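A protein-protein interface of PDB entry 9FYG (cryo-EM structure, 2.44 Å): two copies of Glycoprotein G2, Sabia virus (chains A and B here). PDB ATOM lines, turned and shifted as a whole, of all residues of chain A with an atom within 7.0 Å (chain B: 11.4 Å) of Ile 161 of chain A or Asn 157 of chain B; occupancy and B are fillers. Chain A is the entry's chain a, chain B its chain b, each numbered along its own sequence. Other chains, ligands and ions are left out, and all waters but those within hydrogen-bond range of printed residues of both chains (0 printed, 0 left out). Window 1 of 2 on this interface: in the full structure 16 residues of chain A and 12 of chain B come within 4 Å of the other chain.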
ATOM      1  N   LEU A 156     -13.896  27.858   6.889  1.00  0.00           N
ATOM      2  CA  LEU A 156     -13.053  26.826   6.310  1.00  0.00           C
ATOM      3  C   LEU A 156     -12.945  25.593   7.194  1.00  0.00           C
ATOM      4  O   LEU A 156     -12.316  24.611   6.789  1.00  0.00           O
ATOM      5  CB  LEU A 156     -11.656  27.385   6.018  1.00  0.00           C
ATOM      6  CG  LEU A 156     -11.388  27.733   4.553  1.00  0.00           C
ATOM      7  CD1 LEU A 156     -12.343  28.812   4.070  1.00  0.00           C
ATOM      8  CD2 LEU A 156      -9.947  28.171   4.363  1.00  0.00           C
ATOM      9  N   ASN A 157     -13.541  25.617   8.386  1.00  0.00           N
ATOM     10  CA  ASN A 157     -13.530  24.457   9.267  1.00  0.00           C
ATOM     11  C   ASN A 157     -14.865  23.733   9.314  1.00  0.00           C
ATOM     12  O   ASN A 157     -14.893  22.526   9.570  1.00  0.00           O
ATOM     13  CB  ASN A 157     -13.130  24.869  10.688  1.00  0.00           C
ATOM     14  CG  ASN A 157     -11.632  25.030  10.846  1.00  0.00           C
ATOM     15  OD1 ASN A 157     -11.148  25.451  11.897  1.00  0.00           O
ATOM     16  ND2 ASN A 157     -10.890  24.693   9.801  1.00  0.00           N
ATOM     17  N   LYS A 158     -15.970  24.442   9.075  1.00  0.00           N
ATOM     18  CA  LYS A 158     -17.272  23.788   9.023  1.00  0.00           C
ATOM     19  C   LYS A 158     -17.402  22.898   7.795  1.00  0.00           C
ATOM     20  O   LYS A 158     -18.103  21.880   7.840  1.00  0.00           O
ATOM     21  CB  LYS A 158     -18.386  24.835   9.044  1.00  0.00           C
ATOM     22  CG  LYS A 158     -19.780  24.260   9.234  1.00  0.00           C
ATOM     23  CD  LYS A 158     -20.815  25.363   9.380  1.00  0.00           C
ATOM     24  CE  LYS A 158     -22.202  24.790   9.617  1.00  0.00           C
ATOM     25  NZ  LYS A 158     -22.670  23.980   8.459  1.00  0.00           N
ATOM     26  N   GLU A 159     -16.742  23.264   6.693  1.00  0.00           N
ATOM     27  CA  GLU A 159     -16.811  22.453   5.481  1.00  0.00           C
ATOM     28  C   GLU A 159     -16.215  21.070   5.706  1.00  0.00           C
ATOM     29  O   GLU A 159     -16.775  20.063   5.256  1.00  0.00           O
ATOM     30  CB  GLU A 159     -16.096  23.166   4.333  1.00  0.00           C
ATOM     31  CG  GLU A 159     -16.866  24.347   3.762  1.00  0.00           C
ATOM     32  CD  GLU A 159     -16.041  25.163   2.788  1.00  0.00           C
ATOM     33  OE1 GLU A 159     -14.870  24.801   2.548  1.00  0.00           O
ATOM     34  OE2 GLU A 159     -16.562  26.170   2.264  1.00  0.00           O
ATOM     35  N   TYR A 160     -15.074  20.999   6.399  1.00  0.00           N
ATOM     36  CA  TYR A 160     -14.472  19.705   6.702  1.00  0.00           C
ATOM     37  C   TYR A 160     -15.377  18.871   7.599  1.00  0.00           C
ATOM     38  O   TYR A 160     -15.543  17.666   7.379  1.00  0.00           O
ATOM     39  CB  TYR A 160     -13.108  19.904   7.361  1.00  0.00           C
ATOM     40  CG  TYR A 160     -11.997  20.250   6.400  1.00  0.00           C
ATOM     41  CD1 TYR A 160     -11.390  19.270   5.624  1.00  0.00           C
ATOM     42  CD2 TYR A 160     -11.549  21.557   6.270  1.00  0.00           C
ATOM     43  CE1 TYR A 160     -10.371  19.585   4.745  1.00  0.00           C
ATOM     44  CE2 TYR A 160     -10.531  21.881   5.396  1.00  0.00           C
ATOM     45  CZ  TYR A 160      -9.946  20.893   4.635  1.00  0.00           C
ATOM     46  OH  TYR A 160      -8.933  21.214   3.763  1.00  0.00           O
ATOM     47  N   ILE A 161     -15.971  19.496   8.617  1.00  0.00           N
ATOM     48  CA  ILE A 161     -16.832  18.765   9.541  1.00  0.00           C
ATOM     49  C   ILE A 161     -18.107  18.312   8.840  1.00  0.00           C
ATOM     50  O   ILE A 161     -18.607  17.207   9.084  1.00  0.00           O
ATOM     51  CB  ILE A 161     -17.136  19.627  10.780  1.00  0.00           C
ATOM     52  CG1 ILE A 161     -15.838  19.991  11.503  1.00  0.00           C
ATOM     53  CG2 ILE A 161     -18.081  18.900  11.723  1.00  0.00           C
ATOM     54  CD1 ILE A 161     -16.040  20.886  12.704  1.00  0.00           C
ATOM     55  N   ASP A 162     -18.658  19.156   7.963  1.00  0.00           N
ATOM     56  CA  ASP A 162     -19.871  18.785   7.243  1.00  0.00           C
ATOM     57  C   ASP A 162     -19.642  17.563   6.364  1.00  0.00           C
ATOM     58  O   ASP A 162     -20.470  16.645   6.333  1.00  0.00           O
ATOM     59  CB  ASP A 162     -20.367  19.963   6.405  1.00  0.00           C
ATOM     60  CG  ASP A 162     -21.111  20.993   7.231  1.00  0.00           C
ATOM     61  OD1 ASP A 162     -21.476  20.681   8.384  1.00  0.00           O
ATOM     62  OD2 ASP A 162     -21.332  22.115   6.728  1.00  0.00           O
ATOM     63  N   ARG A 163     -18.522  17.532   5.636  1.00  0.00           N
ATOM     64  CA  ARG A 163     -18.197  16.355   4.836  1.00  0.00           C
ATOM     65  C   ARG A 163     -17.923  15.146   5.721  1.00  0.00           C
ATOM     66  O   ARG A 163     -18.360  14.031   5.412  1.00  0.00           O
ATOM     67  CB  ARG A 163     -16.996  16.648   3.936  1.00  0.00           C
ATOM     68  CG  ARG A 163     -16.367  15.409   3.317  1.00  0.00           C
ATOM     69  CD  ARG A 163     -15.559  15.756   2.079  1.00  0.00           C
ATOM     70  NE  ARG A 163     -16.399  16.289   1.012  1.00  0.00           N
ATOM     71  CZ  ARG A 163     -15.978  16.527  -0.222  1.00  0.00           C
ATOM     72  NH1 ARG A 163     -14.728  16.288  -0.585  1.00  0.00           N
ATOM     73  NH2 ARG A 163     -16.832  17.018  -1.116  1.00  0.00           N
ATOM     74  N   GLN A 164     -17.203  15.348   6.827  1.00  0.00           N
ATOM     75  CA  GLN A 164     -16.914  14.244   7.737  1.00  0.00           C
ATOM     76  C   GLN A 164     -18.179  13.707   8.393  1.00  0.00           C
ATOM     77  O   GLN A 164     -18.238  12.523   8.745  1.00  0.00           O
ATOM     78  CB  GLN A 164     -15.911  14.691   8.801  1.00  0.00           C
ATOM     79  CG  GLN A 164     -14.475  14.768   8.304  1.00  0.00           C
ATOM     80  CD  GLN A 164     -13.522  15.302   9.354  1.00  0.00           C
ATOM     81  OE1 GLN A 164     -13.892  15.472  10.516  1.00  0.00           O
ATOM     82  NE2 GLN A 164     -12.286  15.570   8.950  1.00  0.00           N
ATOM     83  N   GLY A 165     -19.191  14.557   8.574  1.00  0.00           N
ATOM     84  CA  GLY A 165     -20.442  14.090   9.149  1.00  0.00           C
ATOM     85  C   GLY A 165     -21.185  13.123   8.245  1.00  0.00           C
ATOM     86  O   GLY A 165     -21.829  12.185   8.722  1.00  0.00           O
ATOM     87  N   LYS A 166     -21.111  13.339   6.932  1.00  0.00           N
ATOM     88  CA  LYS A 166     -21.838  12.516   5.974  1.00  0.00           C
ATOM     89  C   LYS A 166     -21.066  11.259   5.581  1.00  0.00           C
ATOM     90  O   LYS A 166     -21.636  10.166   5.538  1.00  0.00           O
ATOM     91  CB  LYS A 166     -22.170  13.339   4.724  1.00  0.00           C
ATOM     92  CG  LYS A 166     -22.759  14.708   5.017  1.00  0.00           C
ATOM     93  CD  LYS A 166     -22.694  15.606   3.793  1.00  0.00           C
ATOM     94  CE  LYS A 166     -23.073  17.038   4.137  1.00  0.00           C
ATOM     95  NZ  LYS A 166     -22.900  17.951   2.974  1.00  0.00           N
ATOM     96  N   THR A 167     -19.770  11.399   5.285  1.00  0.00           N
ATOM     97  CA  THR A 167     -18.966  10.277   4.813  1.00  0.00           C
ATOM     98  C   THR A 167     -18.246   9.614   5.976  1.00  0.00           C
ATOM     99  O   THR A 167     -17.544  10.299   6.733  1.00  0.00           O
ATOM    100  CB  THR A 167     -17.948  10.742   3.776  1.00  0.00           C
ATOM    101  OG1 THR A 167     -17.108  11.751   4.347  1.00  0.00           O
ATOM    102  CG2 THR A 167     -18.657  11.310   2.555  1.00  0.00           C
ATOM    103  N   THR B  37     -19.254   9.125  26.917  1.00  0.00           N
ATOM    104  CA  THR B  37     -19.301  10.012  25.758  1.00  0.00           C
ATOM    105  C   THR B  37     -20.528  10.914  25.803  1.00  0.00           C
ATOM    106  O   THR B  37     -20.436  12.114  25.517  1.00  0.00           O
ATOM    107  CB  THR B  37     -19.287   9.193  24.467  1.00  0.00           C
ATOM    108  OG1 THR B  37     -18.213   8.246  24.510  1.00  0.00           O
ATOM    109  CG2 THR B  37     -19.105  10.102  23.262  1.00  0.00           C
ATOM    110  N   LYS B  41     -21.176  15.799  28.062  1.00  0.00           N
ATOM    111  CA  LYS B  41     -21.834  17.057  27.738  1.00  0.00           C
ATOM    112  C   LYS B  41     -22.485  17.714  28.947  1.00  0.00           C
ATOM    113  O   LYS B  41     -22.979  18.840  28.825  1.00  0.00           O
ATOM    114  CB  LYS B  41     -22.890  16.834  26.654  1.00  0.00           C
ATOM    115  CG  LYS B  41     -22.498  15.814  25.599  1.00  0.00           C
ATOM    116  CD  LYS B  41     -23.596  15.651  24.562  1.00  0.00           C
ATOM    117  CE  LYS B  41     -23.354  14.437  23.680  1.00  0.00           C
ATOM    118  NZ  LYS B  41     -22.164  14.614  22.807  1.00  0.00           N
ATOM    119  N   GLU B 120     -24.390   3.255  21.221  1.00  0.00           N
ATOM    120  CA  GLU B 120     -24.185   4.675  21.461  1.00  0.00           C
ATOM    121  C   GLU B 120     -25.524   5.391  21.576  1.00  0.00           C
ATOM    122  O   GLU B 120     -26.519   5.002  20.958  1.00  0.00           O
ATOM    123  CB  GLU B 120     -23.349   5.294  20.341  1.00  0.00           C
ATOM    124  CG  GLU B 120     -22.070   4.537  20.030  1.00  0.00           C
ATOM    125  CD  GLU B 120     -21.011   4.719  21.101  1.00  0.00           C
ATOM    126  OE1 GLU B 120     -20.703   5.879  21.444  1.00  0.00           O
ATOM    127  OE2 GLU B 120     -20.487   3.700  21.599  1.00  0.00           O
ATOM    128  N   GLU B 147     -32.061  15.288  16.634  1.00  0.00           N
ATOM    129  CA  GLU B 147     -31.189  14.680  17.636  1.00  0.00           C
ATOM    130  C   GLU B 147     -30.639  13.350  17.140  1.00  0.00           C
ATOM    131  O   GLU B 147     -29.423  13.121  17.158  1.00  0.00           O
ATOM    132  CB  GLU B 147     -31.952  14.486  18.947  1.00  0.00           C
ATOM    133  CG  GLU B 147     -31.110  13.944  20.089  1.00  0.00           C
ATOM    134  CD  GLU B 147     -30.586  15.037  20.994  1.00  0.00           C
ATOM    135  OE1 GLU B 147     -31.201  16.122  21.037  1.00  0.00           O
ATOM    136  OE2 GLU B 147     -29.559  14.813  21.666  1.00  0.00           O
ATOM    137  N   SER B 148     -31.522  12.480  16.639  1.00  0.00           N
ATOM    138  CA  SER B 148     -31.071  11.196  16.115  1.00  0.00           C
ATOM    139  C   SER B 148     -30.034  11.401  15.021  1.00  0.00           C
ATOM    140  O   SER B 148     -28.963  10.783  15.040  1.00  0.00           O
ATOM    141  CB  SER B 148     -32.264  10.396  15.593  1.00  0.00           C
ATOM    142  OG  SER B 148     -31.840   9.315  14.782  1.00  0.00           O
ATOM    143  N   ASP B 149     -30.317  12.319  14.092  1.00  0.00           N
ATOM    144  CA  ASP B 149     -29.349  12.649  13.054  1.00  0.00           C
ATOM    145  C   ASP B 149     -28.004  12.997  13.670  1.00  0.00           C
ATOM    146  O   ASP B 149     -26.971  12.421  13.304  1.00  0.00           O
ATOM    147  CB  ASP B 149     -29.869  13.807  12.200  1.00  0.00           C
ATOM    148  CG  ASP B 149     -31.144  13.458  11.458  1.00  0.00           C
ATOM    149  OD1 ASP B 149     -31.410  12.255  11.260  1.00  0.00           O
ATOM    150  OD2 ASP B 149     -31.882  14.391  11.075  1.00  0.00           O
ATOM    151  N   HIS B 150     -28.011  13.896  14.662  1.00  0.00           N
ATOM    152  CA  HIS B 150     -26.761  14.291  15.299  1.00  0.00           C
ATOM    153  C   HIS B 150     -26.007  13.074  15.807  1.00  0.00           C
ATOM    154  O   HIS B 150     -24.799  12.945  15.576  1.00  0.00           O
ATOM    155  CB  HIS B 150     -27.024  15.269  16.443  1.00  0.00           C
ATOM    156  CG  HIS B 150     -27.381  16.649  15.990  1.00  0.00           C
ATOM    157  ND1 HIS B 150     -26.484  17.478  15.352  1.00  0.00           N
ATOM    158  CD2 HIS B 150     -28.531  17.353  16.100  1.00  0.00           C
ATOM    159  CE1 HIS B 150     -27.071  18.629  15.077  1.00  0.00           C
ATOM    160  NE2 HIS B 150     -28.314  18.580  15.521  1.00  0.00           N
ATOM    161  N   LEU B 151     -26.722  12.142  16.447  1.00  0.00           N
ATOM    162  CA  LEU B 151     -26.072  10.940  16.952  1.00  0.00           C
ATOM    163  C   LEU B 151     -25.296  10.253  15.842  1.00  0.00           C
ATOM    164  O   LEU B 151     -24.085  10.024  15.962  1.00  0.00           O
ATOM    165  CB  LEU B 151     -27.112   9.994  17.557  1.00  0.00           C
ATOM    166  CG  LEU B 151     -26.570   8.713  18.193  1.00  0.00           C
ATOM    167  CD1 LEU B 151     -25.814   9.030  19.470  1.00  0.00           C
ATOM    168  CD2 LEU B 151     -27.695   7.729  18.459  1.00  0.00           C
ATOM    169  N   LEU B 152     -25.962   9.997  14.713  1.00  0.00           N
ATOM    170  CA  LEU B 152     -25.280   9.361  13.594  1.00  0.00           C
ATOM    171  C   LEU B 152     -24.097  10.203  13.146  1.00  0.00           C
ATOM    172  O   LEU B 152     -22.981   9.693  12.984  1.00  0.00           O
ATOM    173  CB  LEU B 152     -26.259   9.134  12.443  1.00  0.00           C
ATOM    174  CG  LEU B 152     -27.555   8.410  12.813  1.00  0.00           C
ATOM    175  CD1 LEU B 152     -28.386   8.125  11.575  1.00  0.00           C
ATOM    176  CD2 LEU B 152     -27.249   7.124  13.562  1.00  0.00           C
ATOM    177  N   SER B 153     -24.308  11.516  13.015  1.00  0.00           N
ATOM    178  CA  SER B 153     -23.209  12.395  12.637  1.00  0.00           C
ATOM    179  C   SER B 153     -22.083  12.306  13.653  1.00  0.00           C
ATOM    180  O   SER B 153     -20.907  12.212  13.282  1.00  0.00           O
ATOM    181  CB  SER B 153     -23.707  13.832  12.500  1.00  0.00           C
ATOM    182  OG  SER B 153     -22.624  14.735  12.359  1.00  0.00           O
ATOM    183  N   GLU B 154     -22.429  12.283  14.943  1.00  0.00           N
ATOM    184  CA  GLU B 154     -21.402  12.134  15.965  1.00  0.00           C
ATOM    185  C   GLU B 154     -20.667  10.814  15.790  1.00  0.00           C
ATOM    186  O   GLU B 154     -19.434  10.764  15.868  1.00  0.00           O
ATOM    187  CB  GLU B 154     -22.025  12.234  17.356  1.00  0.00           C
ATOM    188  CG  GLU B 154     -21.020  12.203  18.493  1.00  0.00           C
ATOM    189  CD  GLU B 154     -21.673  12.372  19.851  1.00  0.00           C
ATOM    190  OE1 GLU B 154     -22.915  12.491  19.905  1.00  0.00           O
ATOM    191  OE2 GLU B 154     -20.944  12.389  20.864  1.00  0.00           O
ATOM    192  N   MET B 155     -21.408   9.740  15.499  1.00  0.00           N
ATOM    193  CA  MET B 155     -20.772   8.449  15.279  1.00  0.00           C
ATOM    194  C   MET B 155     -19.886   8.457  14.045  1.00  0.00           C
ATOM    195  O   MET B 155     -18.987   7.616  13.937  1.00  0.00           O
ATOM    196  CB  MET B 155     -21.832   7.354  15.163  1.00  0.00           C
ATOM    197  CG  MET B 155     -22.424   6.925  16.496  1.00  0.00           C
ATOM    198  SD  MET B 155     -23.617   5.584  16.335  1.00  0.00           S
ATOM    199  CE  MET B 155     -22.955   4.710  14.919  1.00  0.00           C
ATOM    200  N   LEU B 156     -20.115   9.383  13.117  1.00  0.00           N
ATOM    201  CA  LEU B 156     -19.261   9.537  11.950  1.00  0.00           C
ATOM    202  C   LEU B 156     -18.227  10.639  12.122  1.00  0.00           C
ATOM    203  O   LEU B 156     -17.390  10.827  11.234  1.00  0.00           O
ATOM    204  CB  LEU B 156     -20.111   9.808  10.704  1.00  0.00           C
ATOM    205  CG  LEU B 156     -20.322   8.601   9.786  1.00  0.00           C
ATOM    206  CD1 LEU B 156     -21.076   7.496  10.510  1.00  0.00           C
ATOM    207  CD2 LEU B 156     -21.061   9.010   8.525  1.00  0.00           C
ATOM    208  N   ASN B 157     -18.263  11.370  13.236  1.00  0.00           N
ATOM    209  CA  ASN B 157     -17.274  12.408  13.496  1.00  0.00           C
ATOM    210  C   ASN B 157     -16.230  11.993  14.519  1.00  0.00           C
ATOM    211  O   ASN B 157     -15.103  12.498  14.477  1.00  0.00           O
ATOM    212  CB  ASN B 157     -17.960  13.693  13.969  1.00  0.00           C
ATOM    213  CG  ASN B 157     -18.515  14.512  12.821  1.00  0.00           C
ATOM    214  OD1 ASN B 157     -19.185  15.523  13.029  1.00  0.00           O
ATOM    215  ND2 ASN B 157     -18.236  14.077  11.598  1.00  0.00           N
ATOM    216  N   LYS B 158     -16.578  11.089  15.437  1.00  0.00           N
ATOM    217  CA  LYS B 158     -15.597  10.594  16.396  1.00  0.00           C
ATOM    218  C   LYS B 158     -14.551   9.717  15.721  1.00  0.00           C
ATOM    219  O   LYS B 158     -13.399   9.675  16.167  1.00  0.00           O
ATOM    220  CB  LYS B 158     -16.300   9.822  17.513  1.00  0.00           C
ATOM    221  CG  LYS B 158     -15.406   9.476  18.691  1.00  0.00           C
ATOM    222  CD  LYS B 158     -16.204   8.842  19.819  1.00  0.00           C
ATOM    223  CE  LYS B 158     -15.320   8.540  21.017  1.00  0.00           C
ATOM    224  NZ  LYS B 158     -14.266   7.542  20.688  1.00  0.00           N
ATOM    225  N   GLU B 159     -14.932   9.009  14.654  1.00  0.00           N
ATOM    226  CA  GLU B 159     -13.980   8.154  13.952  1.00  0.00           C
ATOM    227  C   GLU B 159     -12.846   8.969  13.344  1.00  0.00           C
ATOM    228  O   GLU B 159     -11.677   8.572  13.419  1.00  0.00           O
ATOM    229  CB  GLU B 159     -14.700   7.346  12.873  1.00  0.00           C
ATOM    230  CG  GLU B 159     -15.552   6.209  13.414  1.00  0.00           C
ATOM    231  CD  GLU B 159     -16.430   5.580  12.351  1.00  0.00           C
ATOM    232  OE1 GLU B 159     -16.365   6.025  11.186  1.00  0.00           O
ATOM    233  OE2 GLU B 159     -17.186   4.643  12.681  1.00  0.00           O
ATOM    234  N   TYR B 160     -13.172  10.111  12.732  1.00  0.00           N
ATOM    235  CA  TYR B 160     -12.136  10.973  12.173  1.00  0.00           C
ATOM    236  C   TYR B 160     -11.219  11.513  13.262  1.00  0.00           C
ATOM    237  O   TYR B 160      -9.994  11.549  13.093  1.00  0.00           O
ATOM    238  CB  TYR B 160     -12.772  12.124  11.395  1.00  0.00           C
ATOM    239  CG  TYR B 160     -13.280  11.741  10.025  1.00  0.00           C
ATOM    240  CD1 TYR B 160     -12.408  11.601   8.953  1.00  0.00           C
ATOM    241  CD2 TYR B 160     -14.632  11.523   9.802  1.00  0.00           C
ATOM    242  CE1 TYR B 160     -12.871  11.254   7.697  1.00  0.00           C
ATOM    243  CE2 TYR B 160     -15.103  11.175   8.552  1.00  0.00           C
ATOM    244  CZ  TYR B 160     -14.219  11.043   7.504  1.00  0.00           C
ATOM    245  OH  TYR B 160     -14.687  10.696   6.258  1.00  0.00           O
ATOM    246  N   ILE B 161     -11.794  11.939  14.388  1.00  0.00           N
ATOM    247  CA  ILE B 161     -10.989  12.493  15.473  1.00  0.00           C
ATOM    248  C   ILE B 161     -10.124  11.411  16.107  1.00  0.00           C
ATOM    249  O   ILE B 161      -8.969  11.657  16.473  1.00  0.00           O
ATOM    250  CB  ILE B 161     -11.897  13.180  16.509  1.00  0.00           C
ATOM    251  CG1 ILE B 161     -12.674  14.324  15.857  1.00  0.00           C
ATOM    252  CG2 ILE B 161     -11.080  13.697  17.683  1.00  0.00           C
ATOM    253  CD1 ILE B 161     -13.636  15.021  16.793  1.00  0.00           C
ATOM    254  N   ASP B 162     -10.666  10.198  16.248  1.00  0.00           N
ATOM    255  CA  ASP B 162      -9.890   9.106  16.828  1.00  0.00           C
ATOM    256  C   ASP B 162      -8.671   8.781  15.974  1.00  0.00           C
ATOM    257  O   ASP B 162      -7.569   8.588  16.501  1.00  0.00           O
ATOM    258  CB  ASP B 162     -10.771   7.869  17.000  1.00  0.00           C
ATOM    259  CG  ASP B 162     -11.665   7.956  18.220  1.00  0.00           C
ATOM    260  OD1 ASP B 162     -11.419   8.829  19.078  1.00  0.00           O
ATOM    261  OD2 ASP B 162     -12.616   7.152  18.321  1.00  0.00           O
ATOM    262  N   ARG B 163      -8.849   8.710  14.653  1.00  0.00           N
ATOM    263  CA  ARG B 163      -7.710   8.484  13.767  1.00  0.00           C
ATOM    264  C   ARG B 163      -6.741   9.659  13.804  1.00  0.00           C
ATOM    265  O   ARG B 163      -5.520   9.465  13.828  1.00  0.00           O
ATOM    266  CB  ARG B 163      -8.195   8.228  12.341  1.00  0.00           C
ATOM    267  CG  ARG B 163      -7.103   8.319  11.288  1.00  0.00           C
ATOM    268  CD  ARG B 163      -7.483   7.561  10.027  1.00  0.00           C
ATOM    269  NE  ARG B 163      -7.634   6.132  10.274  1.00  0.00           N
ATOM    270  CZ  ARG B 163      -7.797   5.221   9.325  1.00  0.00           C
ATOM    271  NH1 ARG B 163      -7.833   5.556   8.045  1.00  0.00           N
ATOM    272  NH2 ARG B 163      -7.928   3.942   9.667  1.00  0.00           N
ATOM    273  N   GLN B 164      -7.267  10.887  13.812  1.00  0.00           N
ATOM    274  CA  GLN B 164      -6.408  12.063  13.870  1.00  0.00           C
ATOM    275  C   GLN B 164      -5.651  12.144  15.189  1.00  0.00           C
ATOM    276  O   GLN B 164      -4.550  12.704  15.237  1.00  0.00           O
ATOM    277  CB  GLN B 164      -7.238  13.329  13.653  1.00  0.00           C
ATOM    278  CG  GLN B 164      -7.640  13.565  12.205  1.00  0.00           C
ATOM    279  CD  GLN B 164      -8.523  14.786  12.036  1.00  0.00           C
ATOM    280  OE1 GLN B 164      -8.712  15.564  12.970  1.00  0.00           O
ATOM    281  NE2 GLN B 164      -9.068  14.960  10.839  1.00  0.00           N
ATOM    282  N   GLY B 165      -6.225  11.603  16.265  1.00  0.00           N
ATOM    283  CA  GLY B 165      -5.528  11.605  17.541  1.00  0.00           C
ATOM    284  C   GLY B 165      -4.290  10.729  17.541  1.00  0.00           C
ATOM    285  O   GLY B 165      -3.291  11.053  18.189  1.00  0.00           O
ATOM    286  N   LYS B 166      -4.336   9.610  16.819  1.00  0.00           N
ATOM    287  CA  LYS B 166      -3.230   8.659  16.802  1.00  0.00           C
ATOM    288  C   LYS B 166      -2.187   9.002  15.743  1.00  0.00           C
ATOM    289  O   LYS B 166      -0.985   8.970  16.021  1.00  0.00           O
ATOM    290  CB  LYS B 166      -3.763   7.241  16.573  1.00  0.00           C
ATOM    291  CG  LYS B 166      -4.951   6.871  17.445  1.00  0.00           C
ATOM    292  CD  LYS B 166      -5.667   5.645  16.902  1.00  0.00           C
ATOM    293  CE  LYS B 166      -6.980   5.404  17.629  1.00  0.00           C
ATOM    294  NZ  LYS B 166      -7.749   4.283  17.025  1.00  0.00           N
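Gln 164 of chain A touches Tyr 160 of chain B, but with the chains exchanged Tyr 160 of chain A does not touch Gln 164 of chain B (7.2 Å).
Gln 164 of chain B touches its own counterpart, Gln 164 of chain A.
Gly 165 of chain A touches Asn 157 of chain B, but with the chains exchanged Asn 157 of chain A does not touch Gly 165 of chain B (15.3 Å).
Lys 166 of chain A touches Leu 156 of chain B, but with the chains exchanged Leu 156 of chain A does not touch Lys 166 of chain B (19.7 Å).
Of the 11 pairs that touch across the chains among the printed residues, 1 has its exchanged pair printed and touching as well.
Of chain B, only Asn 157 comes within 4 Å of Ile 161 of chain A.
Asn 157 of chain B touches three residues of chain A.
No residue of chain B comes within 4 Å of Asn 157 of chain A.
Of chain B, only Leu 156, Asn 157, Tyr 160 and Gln 164 come within 4 Å of Gln 164 of chain A.
Of chain B, only Ser 153, Leu 156 and Asn 157 come within 4 Å of Gly 165 of chain A.
Printed residues of chain A within 4 Å of Ser 153 of chain B: Gly 165.
Of the printed residues of chain A, Leu 156 of chain B touches Gln 164 (3.1 Å), Gly 165 (3.3 Å), Lys 166 (3.3 Å) and Thr 167 (3.8 Å).
Of the printed residues of chain B, Thr 167 of chain A touches Leu 156 (3.8 Å) and Tyr 160 (2.9 Å).
Of the printed residues of chain B, Lys 166 of chain A touches Leu 156.
Lys 41 of chain B touches none of the printed residues of chain A.
Arg 163 of chain B touches none of the printed residues of chain A.
The nearest residue of chain B that does not touch Ile 161 of chain A is Ser 153 of chain B (5.7 Å).
The side-chain hydroxyl (OG1) of Thr 167 of chain A lies within hydrogen-bond range of the backbone carbonyl oxygen (O) of Arg 163 of chain A, 2.8 Å away.
The side-chain amide nitrogen (ND2) of Asn 157 of chain B sits close to the backbone carbonyl oxygen (O) of Gln 164 of chain A, 3.2 Å away.
N of Gly 165 of chain A sits close to ND2 of Asn 157 of chain B, 3.2 Å away.
The backbone carbonyl oxygen of Thr 167 of chain A lies within hydrogen-bond range of the side-chain hydroxyl of Tyr 160 of chain B, 2.9 Å away.
The backbone carbonyl oxygen (O) of Gln 164 of chain A sits close to the backbone carbonyl oxygen (O) of Leu 156 of chain B, at 3.1 Å.
Hydrophobic or aromatic side chains of chain A that line the printed part of chain B: Ile 161.
Along chain A the printed residues that touch a printed residue of chain B span positions 161 to 167.
Among the printed residues, 11 pairs touch across the chains.
Among the printed residues, merely in contact across the chains: Ile 161 of chain A with Asn 157 of chain B (3.8 Å), Gln 164 of chain A with Tyr 160 of chain B (3.4 Å), Gln 164 of chain A with Gln 164 of chain B (3.8 Å), Gly 165 of chain A with Ser 153 of chain B (3.9 Å), Gly 165 of chain A with Leu 156 of chain B (3.3 Å), Lys 166 of chain A with Leu 156 of chain B (3.3 Å) and Thr 167 of chain A with Leu 156 of chain B (3.8 Å).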
